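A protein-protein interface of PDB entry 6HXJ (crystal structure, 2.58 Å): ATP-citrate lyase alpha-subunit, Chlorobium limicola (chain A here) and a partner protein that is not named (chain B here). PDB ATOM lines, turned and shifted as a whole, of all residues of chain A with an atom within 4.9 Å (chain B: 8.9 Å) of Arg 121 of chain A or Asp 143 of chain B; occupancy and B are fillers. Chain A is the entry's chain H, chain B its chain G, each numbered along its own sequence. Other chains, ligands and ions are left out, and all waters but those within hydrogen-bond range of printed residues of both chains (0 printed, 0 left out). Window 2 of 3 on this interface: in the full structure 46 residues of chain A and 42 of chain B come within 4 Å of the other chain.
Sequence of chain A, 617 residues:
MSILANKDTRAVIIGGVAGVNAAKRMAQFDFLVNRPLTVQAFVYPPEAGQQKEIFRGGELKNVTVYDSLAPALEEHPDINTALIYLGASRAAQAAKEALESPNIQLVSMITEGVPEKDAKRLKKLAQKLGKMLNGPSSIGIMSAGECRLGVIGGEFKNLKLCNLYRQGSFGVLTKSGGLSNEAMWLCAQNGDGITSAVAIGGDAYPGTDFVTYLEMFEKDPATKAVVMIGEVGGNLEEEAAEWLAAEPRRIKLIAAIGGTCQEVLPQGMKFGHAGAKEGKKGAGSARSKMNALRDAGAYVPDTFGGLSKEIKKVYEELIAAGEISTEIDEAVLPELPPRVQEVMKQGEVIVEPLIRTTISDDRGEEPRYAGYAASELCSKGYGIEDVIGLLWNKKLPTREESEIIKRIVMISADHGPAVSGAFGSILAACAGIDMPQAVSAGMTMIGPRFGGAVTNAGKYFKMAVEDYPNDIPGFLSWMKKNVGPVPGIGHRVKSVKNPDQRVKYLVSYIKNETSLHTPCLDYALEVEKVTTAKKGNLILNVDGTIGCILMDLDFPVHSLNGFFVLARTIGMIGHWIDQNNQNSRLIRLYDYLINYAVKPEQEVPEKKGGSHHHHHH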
ATOM      1  N   LYS A 117      -9.605   7.597 -28.796  1.00  0.00           N
ATOM      2  CA  LYS A 117      -9.795   8.965 -29.291  1.00  0.00           C
ATOM      3  C   LYS A 117      -9.759   8.993 -30.846  1.00  0.00           C
ATOM      4  O   LYS A 117     -10.602   9.642 -31.463  1.00  0.00           O
ATOM      5  CB  LYS A 117      -8.740   9.904 -28.688  1.00  0.00           C
ATOM      6  CG  LYS A 117      -9.035  11.391 -28.887  1.00  0.00           C
ATOM      7  CD  LYS A 117      -7.953  12.253 -28.226  1.00  0.00           C
ATOM      8  CE  LYS A 117      -8.238  13.727 -28.357  1.00  0.00           C
ATOM      9  NZ  LYS A 117      -6.986  14.533 -28.374  1.00  0.00           N
ATOM     10  N   ASP A 118      -8.839   8.234 -31.464  1.00  0.00           N
ATOM     11  CA  ASP A 118      -8.725   8.144 -32.923  1.00  0.00           C
ATOM     12  C   ASP A 118      -9.901   7.442 -33.566  1.00  0.00           C
ATOM     13  O   ASP A 118     -10.412   7.936 -34.565  1.00  0.00           O
ATOM     14  CB  ASP A 118      -7.405   7.497 -33.342  1.00  0.00           C
ATOM     15  CG  ASP A 118      -6.156   8.326 -33.048  1.00  0.00           C
ATOM     16  OD1 ASP A 118      -6.285   9.406 -32.381  1.00  0.00           O
ATOM     17  OD2 ASP A 118      -5.039   7.900 -33.478  1.00  0.00           O
ATOM     18  N   ALA A 119     -10.346   6.306 -32.995  1.00  0.00           N
ATOM     19  CA  ALA A 119     -11.494   5.539 -33.473  1.00  0.00           C
ATOM     20  C   ALA A 119     -12.767   6.368 -33.381  1.00  0.00           C
ATOM     21  O   ALA A 119     -13.561   6.330 -34.314  1.00  0.00           O
ATOM     22  CB  ALA A 119     -11.644   4.257 -32.675  1.00  0.00           C
ATOM     23  N   LYS A 120     -12.942   7.149 -32.297  1.00  0.00           N
ATOM     24  CA  LYS A 120     -14.107   8.031 -32.087  1.00  0.00           C
ATOM     25  C   LYS A 120     -14.178   9.115 -33.171  1.00  0.00           C
ATOM     26  O   LYS A 120     -15.247   9.333 -33.747  1.00  0.00           O
ATOM     27  CB  LYS A 120     -14.071   8.666 -30.693  1.00  0.00           C
ATOM     28  CG  LYS A 120     -14.515   7.737 -29.584  1.00  0.00           C
ATOM     29  CD  LYS A 120     -14.818   8.530 -28.334  1.00  0.00           C
ATOM     30  CE  LYS A 120     -13.873   8.211 -27.212  1.00  0.00           C
ATOM     31  NZ  LYS A 120     -14.161   8.981 -25.961  1.00  0.00           N
ATOM     32  N   ARG A 121     -13.029   9.759 -33.457  1.00  0.00           N
ATOM     33  CA  ARG A 121     -12.840  10.762 -34.511  1.00  0.00           C
ATOM     34  C   ARG A 121     -13.143  10.181 -35.917  1.00  0.00           C
ATOM     35  O   ARG A 121     -13.821  10.839 -36.710  1.00  0.00           O
ATOM     36  CB  ARG A 121     -11.403  11.322 -34.456  1.00  0.00           C
ATOM     37  CG  ARG A 121     -11.267  12.439 -33.430  1.00  0.00           C
ATOM     38  CD  ARG A 121      -9.832  12.836 -33.219  1.00  0.00           C
ATOM     39  NE  ARG A 121      -9.731  14.065 -32.437  1.00  0.00           N
ATOM     40  CZ  ARG A 121      -8.607  14.490 -31.874  1.00  0.00           C
ATOM     41  NH1 ARG A 121      -8.592  15.626 -31.184  1.00  0.00           N
ATOM     42  NH2 ARG A 121      -7.490  13.785 -31.991  1.00  0.00           N
ATOM     43  N   LEU A 122     -12.676   8.950 -36.213  1.00  0.00           N
ATOM     44  CA  LEU A 122     -12.934   8.317 -37.500  1.00  0.00           C
ATOM     45  C   LEU A 122     -14.395   7.906 -37.652  1.00  0.00           C
ATOM     46  O   LEU A 122     -14.897   7.907 -38.766  1.00  0.00           O
ATOM     47  CB  LEU A 122     -11.998   7.121 -37.768  1.00  0.00           C
ATOM     48  CG  LEU A 122     -10.514   7.419 -38.045  1.00  0.00           C
ATOM     49  CD1 LEU A 122      -9.669   6.211 -37.777  1.00  0.00           C
ATOM     50  CD2 LEU A 122     -10.283   7.857 -39.470  1.00  0.00           C
ATOM     51  N   LYS A 123     -15.063   7.531 -36.570  1.00  0.00           N
ATOM     52  CA  LYS A 123     -16.475   7.169 -36.626  1.00  0.00           C
ATOM     53  C   LYS A 123     -17.307   8.409 -36.996  1.00  0.00           C
ATOM     54  O   LYS A 123     -18.164   8.304 -37.872  1.00  0.00           O
ATOM     55  CB  LYS A 123     -16.957   6.553 -35.292  1.00  0.00           C
ATOM     56  CG  LYS A 123     -18.397   6.064 -35.327  1.00  0.00           C
ATOM     57  CD  LYS A 123     -18.799   5.344 -34.049  1.00  0.00           C
ATOM     58  CE  LYS A 123     -20.282   5.019 -33.980  1.00  0.00           C
ATOM     59  NZ  LYS A 123     -20.700   3.941 -34.931  1.00  0.00           N
ATOM     60  N   LYS A 124     -17.033   9.576 -36.354  1.00  0.00           N
ATOM     61  CA  LYS A 124     -17.719  10.852 -36.613  1.00  0.00           C
ATOM     62  C   LYS A 124     -17.462  11.359 -38.034  1.00  0.00           C
ATOM     63  O   LYS A 124     -18.385  11.862 -38.660  1.00  0.00           O
ATOM     64  CB  LYS A 124     -17.364  11.929 -35.565  1.00  0.00           C
ATOM     65  CG  LYS A 124     -17.930  11.694 -34.153  1.00  0.00           C
ATOM     66  CD  LYS A 124     -19.427  12.051 -34.011  1.00  0.00           C
ATOM     67  CE  LYS A 124     -19.929  11.957 -32.587  1.00  0.00           C
ATOM     68  NZ  LYS A 124     -19.490  13.125 -31.772  1.00  0.00           N
ATOM     69  N   LEU A 125     -16.228  11.191 -38.549  1.00  0.00           N
ATOM     70  CA  LEU A 125     -15.874  11.563 -39.923  1.00  0.00           C
ATOM     71  C   LEU A 125     -16.655  10.714 -40.924  1.00  0.00           C
ATOM     72  O   LEU A 125     -17.198  11.265 -41.870  1.00  0.00           O
ATOM     73  CB  LEU A 125     -14.361  11.454 -40.158  1.00  0.00           C
ATOM     74  CG  LEU A 125     -13.845  11.766 -41.553  1.00  0.00           C
ATOM     75  CD1 LEU A 125     -13.866  13.245 -41.825  1.00  0.00           C
ATOM     76  CD2 LEU A 125     -12.434  11.250 -41.746  1.00  0.00           C
ATOM     77  N   ASN B 112     -17.543   8.311 -23.823  1.00  0.00           N
ATOM     78  CA  ASN B 112     -18.593   7.593 -24.537  1.00  0.00           C
ATOM     79  C   ASN B 112     -18.372   7.656 -26.059  1.00  0.00           C
ATOM     80  O   ASN B 112     -17.428   8.310 -26.500  1.00  0.00           O
ATOM     81  CB  ASN B 112     -19.987   8.031 -24.108  1.00  0.00           C
ATOM     82  CG  ASN B 112     -20.226   9.498 -24.173  1.00  0.00           C
ATOM     83  OD1 ASN B 112     -20.292  10.102 -25.246  1.00  0.00           O
ATOM     84  ND2 ASN B 112     -20.431  10.085 -23.007  1.00  0.00           N
ATOM     85  N   LYS B 113     -19.218   6.954 -26.851  1.00  0.00           N
ATOM     86  CA  LYS B 113     -19.125   6.889 -28.324  1.00  0.00           C
ATOM     87  C   LYS B 113     -19.130   8.251 -28.991  1.00  0.00           C
ATOM     88  O   LYS B 113     -18.554   8.374 -30.061  1.00  0.00           O
ATOM     89  CB  LYS B 113     -20.253   6.040 -28.940  1.00  0.00           C
ATOM     90  CG  LYS B 113     -20.334   4.608 -28.470  1.00  0.00           C
ATOM     91  CD  LYS B 113     -21.393   3.844 -29.247  1.00  0.00           C
ATOM     92  CE  LYS B 113     -22.818   4.118 -28.814  1.00  0.00           C
ATOM     93  NZ  LYS B 113     -23.761   3.094 -29.342  1.00  0.00           N
ATOM     94  N   ASP B 114     -19.749   9.270 -28.361  1.00  0.00           N
ATOM     95  CA  ASP B 114     -19.884  10.639 -28.879  1.00  0.00           C
ATOM     96  C   ASP B 114     -18.916  11.673 -28.265  1.00  0.00           C
ATOM     97  O   ASP B 114     -18.949  12.840 -28.653  1.00  0.00           O
ATOM     98  CB  ASP B 114     -21.342  11.114 -28.717  1.00  0.00           C
ATOM     99  CG  ASP B 114     -22.387  10.200 -29.336  1.00  0.00           C
ATOM    100  OD1 ASP B 114     -22.178   9.746 -30.494  1.00  0.00           O
ATOM    101  OD2 ASP B 114     -23.437   9.962 -28.679  1.00  0.00           O
ATOM    102  N   GLY B 115     -18.064  11.230 -27.338  1.00  0.00           N
ATOM    103  CA  GLY B 115     -17.105  12.077 -26.636  1.00  0.00           C
ATOM    104  C   GLY B 115     -17.025  11.607 -25.198  1.00  0.00           C
ATOM    105  O   GLY B 115     -16.558  10.494 -24.939  1.00  0.00           O
ATOM    106  N   ALA B 116     -17.471  12.449 -24.251  1.00  0.00           N
ATOM    107  CA  ALA B 116     -17.484  12.150 -22.801  1.00  0.00           C
ATOM    108  C   ALA B 116     -18.600  12.873 -22.050  1.00  0.00           C
ATOM    109  O   ALA B 116     -19.086  13.903 -22.498  1.00  0.00           O
ATOM    110  CB  ALA B 116     -16.135  12.548 -22.215  1.00  0.00           C
ATOM    111  N   GLN B 139     -23.217  16.279 -21.603  1.00  0.00           N
ATOM    112  CA  GLN B 139     -22.478  15.481 -22.568  1.00  0.00           C
ATOM    113  C   GLN B 139     -21.588  16.405 -23.394  1.00  0.00           C
ATOM    114  O   GLN B 139     -22.085  17.307 -24.073  1.00  0.00           O
ATOM    115  CB  GLN B 139     -23.457  14.672 -23.443  1.00  0.00           C
ATOM    116  CG  GLN B 139     -22.927  14.195 -24.809  1.00  0.00           C
ATOM    117  CD  GLN B 139     -21.878  13.121 -24.722  1.00  0.00           C
ATOM    118  OE1 GLN B 139     -21.841  12.324 -23.790  1.00  0.00           O
ATOM    119  NE2 GLN B 139     -21.009  13.063 -25.711  1.00  0.00           N
ATOM    120  N   ILE B 140     -20.270  16.189 -23.306  1.00  0.00           N
ATOM    121  CA  ILE B 140     -19.246  16.930 -24.047  1.00  0.00           C
ATOM    122  C   ILE B 140     -19.025  16.226 -25.371  1.00  0.00           C
ATOM    123  O   ILE B 140     -18.480  15.118 -25.408  1.00  0.00           O
ATOM    124  CB  ILE B 140     -17.931  17.125 -23.236  1.00  0.00           C
ATOM    125  CG1 ILE B 140     -18.207  18.001 -22.012  1.00  0.00           C
ATOM    126  CG2 ILE B 140     -16.828  17.764 -24.095  1.00  0.00           C
ATOM    127  CD1 ILE B 140     -17.757  17.479 -20.828  1.00  0.00           C
ATOM    128  N   GLU B 141     -19.485  16.848 -26.455  1.00  0.00           N
ATOM    129  CA  GLU B 141     -19.293  16.289 -27.782  1.00  0.00           C
ATOM    130  C   GLU B 141     -17.814  16.328 -28.147  1.00  0.00           C
ATOM    131  O   GLU B 141     -17.101  17.251 -27.750  1.00  0.00           O
ATOM    132  CB  GLU B 141     -20.164  17.008 -28.820  1.00  0.00           C
ATOM    133  CG  GLU B 141     -21.607  16.524 -28.819  1.00  0.00           C
ATOM    134  CD  GLU B 141     -21.804  15.039 -29.081  1.00  0.00           C
ATOM    135  OE1 GLU B 141     -21.410  14.557 -30.170  1.00  0.00           O
ATOM    136  OE2 GLU B 141     -22.361  14.359 -28.187  1.00  0.00           O
ATOM    137  N   LEU B 142     -17.347  15.278 -28.825  1.00  0.00           N
ATOM    138  CA  LEU B 142     -15.962  15.086 -29.251  1.00  0.00           C
ATOM    139  C   LEU B 142     -15.410  16.320 -29.981  1.00  0.00           C
ATOM    140  O   LEU B 142     -16.006  16.772 -30.972  1.00  0.00           O
ATOM    141  CB  LEU B 142     -15.899  13.832 -30.132  1.00  0.00           C
ATOM    142  CG  LEU B 142     -14.554  13.329 -30.608  1.00  0.00           C
ATOM    143  CD1 LEU B 142     -13.850  12.541 -29.529  1.00  0.00           C
ATOM    144  CD2 LEU B 142     -14.743  12.455 -31.827  1.00  0.00           C
ATOM    145  N   ASP B 143     -14.310  16.902 -29.426  1.00  0.00           N
ATOM    146  CA  ASP B 143     -13.605  18.101 -29.916  1.00  0.00           C
ATOM    147  C   ASP B 143     -14.472  19.399 -29.898  1.00  0.00           C
ATOM    148  O   ASP B 143     -14.096  20.408 -30.509  1.00  0.00           O
ATOM    149  CB  ASP B 143     -12.977  17.866 -31.323  1.00  0.00           C
ATOM    150  CG  ASP B 143     -12.010  16.699 -31.439  1.00  0.00           C
ATOM    151  OD1 ASP B 143     -11.193  16.502 -30.504  1.00  0.00           O
ATOM    152  OD2 ASP B 143     -12.035  16.010 -32.487  1.00  0.00           O
ATOM    153  N   GLU B 144     -15.617  19.369 -29.189  1.00  0.00           N
ATOM    154  CA  GLU B 144     -16.539  20.503 -29.049  1.00  0.00           C
ATOM    155  C   GLU B 144     -16.667  20.797 -27.562  1.00  0.00           C
ATOM    156  O   GLU B 144     -17.770  20.750 -27.007  1.00  0.00           O
ATOM    157  CB  GLU B 144     -17.912  20.185 -29.683  1.00  0.00           C
ATOM    158  CG  GLU B 144     -17.879  19.976 -31.191  1.00  0.00           C
ATOM    159  CD  GLU B 144     -19.099  19.267 -31.745  1.00  0.00           C
ATOM    160  OE1 GLU B 144     -20.186  19.890 -31.778  1.00  0.00           O
ATOM    161  OE2 GLU B 144     -18.970  18.086 -32.144  1.00  0.00           O
ATOM    162  N   ASN B 145     -15.512  21.063 -26.914  1.00  0.00           N
ATOM    163  CA  ASN B 145     -15.392  21.320 -25.468  1.00  0.00           C
ATOM    164  C   ASN B 145     -16.108  22.616 -25.015  1.00  0.00           C
ATOM    165  O   ASN B 145     -15.968  23.648 -25.683  1.00  0.00           O
ATOM    166  CB  ASN B 145     -13.927  21.283 -25.031  1.00  0.00           C
ATOM    167  CG  ASN B 145     -13.221  19.960 -25.312  1.00  0.00           C
ATOM    168  OD1 ASN B 145     -13.805  18.963 -25.786  1.00  0.00           O
ATOM    169  ND2 ASN B 145     -11.935  19.917 -25.007  1.00  0.00           N
ATOM    170  N   PRO B 146     -16.912  22.563 -23.912  1.00  0.00           N
ATOM    171  CA  PRO B 146     -17.686  23.752 -23.499  1.00  0.00           C
ATOM    172  C   PRO B 146     -16.859  24.915 -22.973  1.00  0.00           C
ATOM    173  O   PRO B 146     -15.691  24.738 -22.621  1.00  0.00           O
ATOM    174  CB  PRO B 146     -18.658  23.205 -22.447  1.00  0.00           C
ATOM    175  CG  PRO B 146     -18.021  21.976 -21.926  1.00  0.00           C
ATOM    176  CD  PRO B 146     -17.190  21.404 -23.031  1.00  0.00           C
ATOM    177  N   ILE B 176     -11.325  18.611 -18.374  1.00  0.00           N
ATOM    178  CA  ILE B 176     -11.670  18.271 -19.752  1.00  0.00           C
ATOM    179  C   ILE B 176     -10.396  18.319 -20.598  1.00  0.00           C
ATOM    180  O   ILE B 176     -10.163  17.416 -21.410  1.00  0.00           O
ATOM    181  CB  ILE B 176     -12.821  19.167 -20.278  1.00  0.00           C
ATOM    182  CG1 ILE B 176     -14.135  18.813 -19.550  1.00  0.00           C
ATOM    183  CG2 ILE B 176     -12.993  19.020 -21.789  1.00  0.00           C
ATOM    184  CD1 ILE B 176     -15.192  19.885 -19.490  1.00  0.00           C
ATOM    185  N   ASP B 180      -9.262  15.021 -22.595  1.00  0.00           N
ATOM    186  CA  ASP B 180      -8.999  15.109 -24.030  1.00  0.00           C
ATOM    187  C   ASP B 180      -7.505  14.929 -24.402  1.00  0.00           C
ATOM    188  O   ASP B 180      -7.204  14.097 -25.267  1.00  0.00           O
ATOM    189  CB  ASP B 180      -9.573  16.418 -24.626  1.00  0.00           C
ATOM    190  CG  ASP B 180     -11.105  16.559 -24.577  1.00  0.00           C
ATOM    191  OD1 ASP B 180     -11.732  16.002 -23.627  1.00  0.00           O
ATOM    192  OD2 ASP B 180     -11.672  17.287 -25.448  1.00  0.00           O
ATOM    193  N   ASN B 181      -6.579  15.657 -23.728  1.00  0.00           N
ATOM    194  CA  ASN B 181      -5.138  15.595 -24.019  1.00  0.00           C
ATOM    195  C   ASN B 181      -4.361  14.390 -23.441  1.00  0.00           C
ATOM    196  O   ASN B 181      -3.268  14.089 -23.944  1.00  0.00           O
ATOM    197  CB  ASN B 181      -4.439  16.872 -23.606  1.00  0.00           C
ATOM    198  CG  ASN B 181      -4.766  18.054 -24.463  1.00  0.00           C
ATOM    199  OD1 ASN B 181      -4.293  18.175 -25.599  1.00  0.00           O
ATOM    200  ND2 ASN B 181      -5.553  18.970 -23.924  1.00  0.00           N
ATOM    201  N   ASP B 183      -5.509  11.195 -23.366  1.00  0.00           N
ATOM    202  CA  ASP B 183      -6.123   9.989 -23.936  1.00  0.00           C
ATOM    203  C   ASP B 183      -6.844   9.159 -22.875  1.00  0.00           C
ATOM    204  O   ASP B 183      -6.761   7.926 -22.865  1.00  0.00           O
ATOM    205  CB  ASP B 183      -5.074   9.153 -24.704  1.00  0.00           C
ATOM    206  CG  ASP B 183      -4.967   9.484 -26.188  1.00  0.00           C
ATOM    207  OD1 ASP B 183      -5.901   9.105 -26.961  1.00  0.00           O
ATOM    208  OD2 ASP B 183      -3.924  10.033 -26.594  1.00  0.00           O
ATOM    209  N   ARG B 217       2.313   8.027 -28.146  1.00  0.00           N
ATOM    210  CA  ARG B 217       2.249   9.467 -28.342  1.00  0.00           C
ATOM    211  C   ARG B 217       2.236  10.260 -26.987  1.00  0.00           C
ATOM    212  O   ARG B 217       1.810  11.425 -26.949  1.00  0.00           O
ATOM    213  CB  ARG B 217       1.085   9.843 -29.288  1.00  0.00           C
ATOM    214  CG  ARG B 217      -0.312   9.567 -28.772  1.00  0.00           C
ATOM    215  CD  ARG B 217      -1.300   9.794 -29.885  1.00  0.00           C
ATOM    216  NE  ARG B 217      -2.675   9.629 -29.429  1.00  0.00           N
ATOM    217  CZ  ARG B 217      -3.739   9.668 -30.224  1.00  0.00           C
ATOM    218  NH1 ARG B 217      -3.595   9.872 -31.527  1.00  0.00           N
ATOM    219  NH2 ARG B 217      -4.957   9.511 -29.720  1.00  0.00           N
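O of Asn 112 of chain B lies close to NZ of Lys 120 of chain A. The side-chain amino group (NZ) of Lys 124 of chain A sits at hydrogen-bond distance from the backbone carbonyl oxygen (O) of Asp 114 of chain B, at 3.2 Å. NZ of Lys 120 of chain A sits at hydrogen-bond distance from O of Gly 115 of chain B. The side-chain carboxylate of Glu 141 of chain B is in salt-bridge range of the side-chain amino group of Lys 124 of chain A, at 2.9 Å. OD1 of Asp 143 of chain B is in salt-bridge range of NH1 of Arg 121 of chain A, at 2.8 Å. O of Asp 180 of chain B is in hydrogen-bond range of NZ of Lys 117 of chain A, at 3.1 Å. The guanidinium group (NH1) of Arg 217 of chain B is in salt-bridge range of the side-chain carboxylate (OD1) of Asp 118 of chain A.
Arg 121 of chain A touches just these residues of chain B: Leu 142 and Asp 143. Of the printed residues of chain B, Lys 124 of chain A touches Asp 114 (3.2 Å) and Glu 141 (2.9 Å). Lys 113 of chain B touches none of the printed residues of chain A. Printed residues of chain A within 4 Å of Gly 115 of chain B: Lys 120. Of the printed residues of chain A, Glu 141 of chain B touches Lys 124 (2.9 Å). Of chain A, only Arg 121 (2.8 Å) comes within 4 Å of Asp 143 of chain B. Glu 144 of chain B touches none of the printed residues of chain A. The nearest residue of chain B that does not touch Arg 121 of chain A is Arg 217 of chain B (5.5 Å). The nearest printed residue of chain B that does not touch Lys 120 of chain A is Lys 113 of chain B (4.1 Å).
Of the 9 printed residues of chain A, 5 touch a printed residue of chain B. Printed residues of chain A that touch a printed residue of chain B: Lys 117, Asp 118, Lys 120, Arg 121 and Lys 124. Hydrophobic or aromatic side chains of chain B that line the printed part of chain A: Leu 142. Among the printed residues, Asp or Glu carboxylates within 4 Å of a Lys or Arg side-chain nitrogen of the other chain: Asp 118 of chain A with Arg 217 of chain B (2.9 Å), Arg 121 of chain A with Asp 143 of chain B (2.8 Å) and Lys 124 of chain A with Glu 141 of chain B (2.9 Å).
N of Asp 114 of chain B sits close to OD1 of Asn 112 of chain B. The side-chain amide oxygen (OD1) of Asn 112 of chain B sits at hydrogen-bond distance from the backbone NH (N) of Gly 115 of chain B (3.3 Å). ND2 of Asn 112 of chain B is in hydrogen-bond range of OE1 of Gln 139 of chain B. The side-chain carboxylate of Glu 141 of chain B lies within hydrogen-bond range of the side-chain amide nitrogen of Gln 139 of chain B (3.1 Å). The side-chain carboxylate (OD2) of Asp 180 of chain B sits at hydrogen-bond distance from the side-chain amide nitrogen (ND2) of Asn 145 of chain B (2.7 Å). OD1 of Asp 183 of chain B is in salt-bridge range of NH2 of Arg 217 of chain B, at 2.9 Å.
Among the printed residues, merely in contact across the chains: Lys 117 of chain A with Asp 183 of chain B (3.4 Å), Arg 121 of chain A with Leu 142 of chain B (3.6 Å), Lys 120 of chain A with Leu 142 of chain B (3.6 Å) and Lys 117 of chain A with Arg 217 of chain B (3.9 Å).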
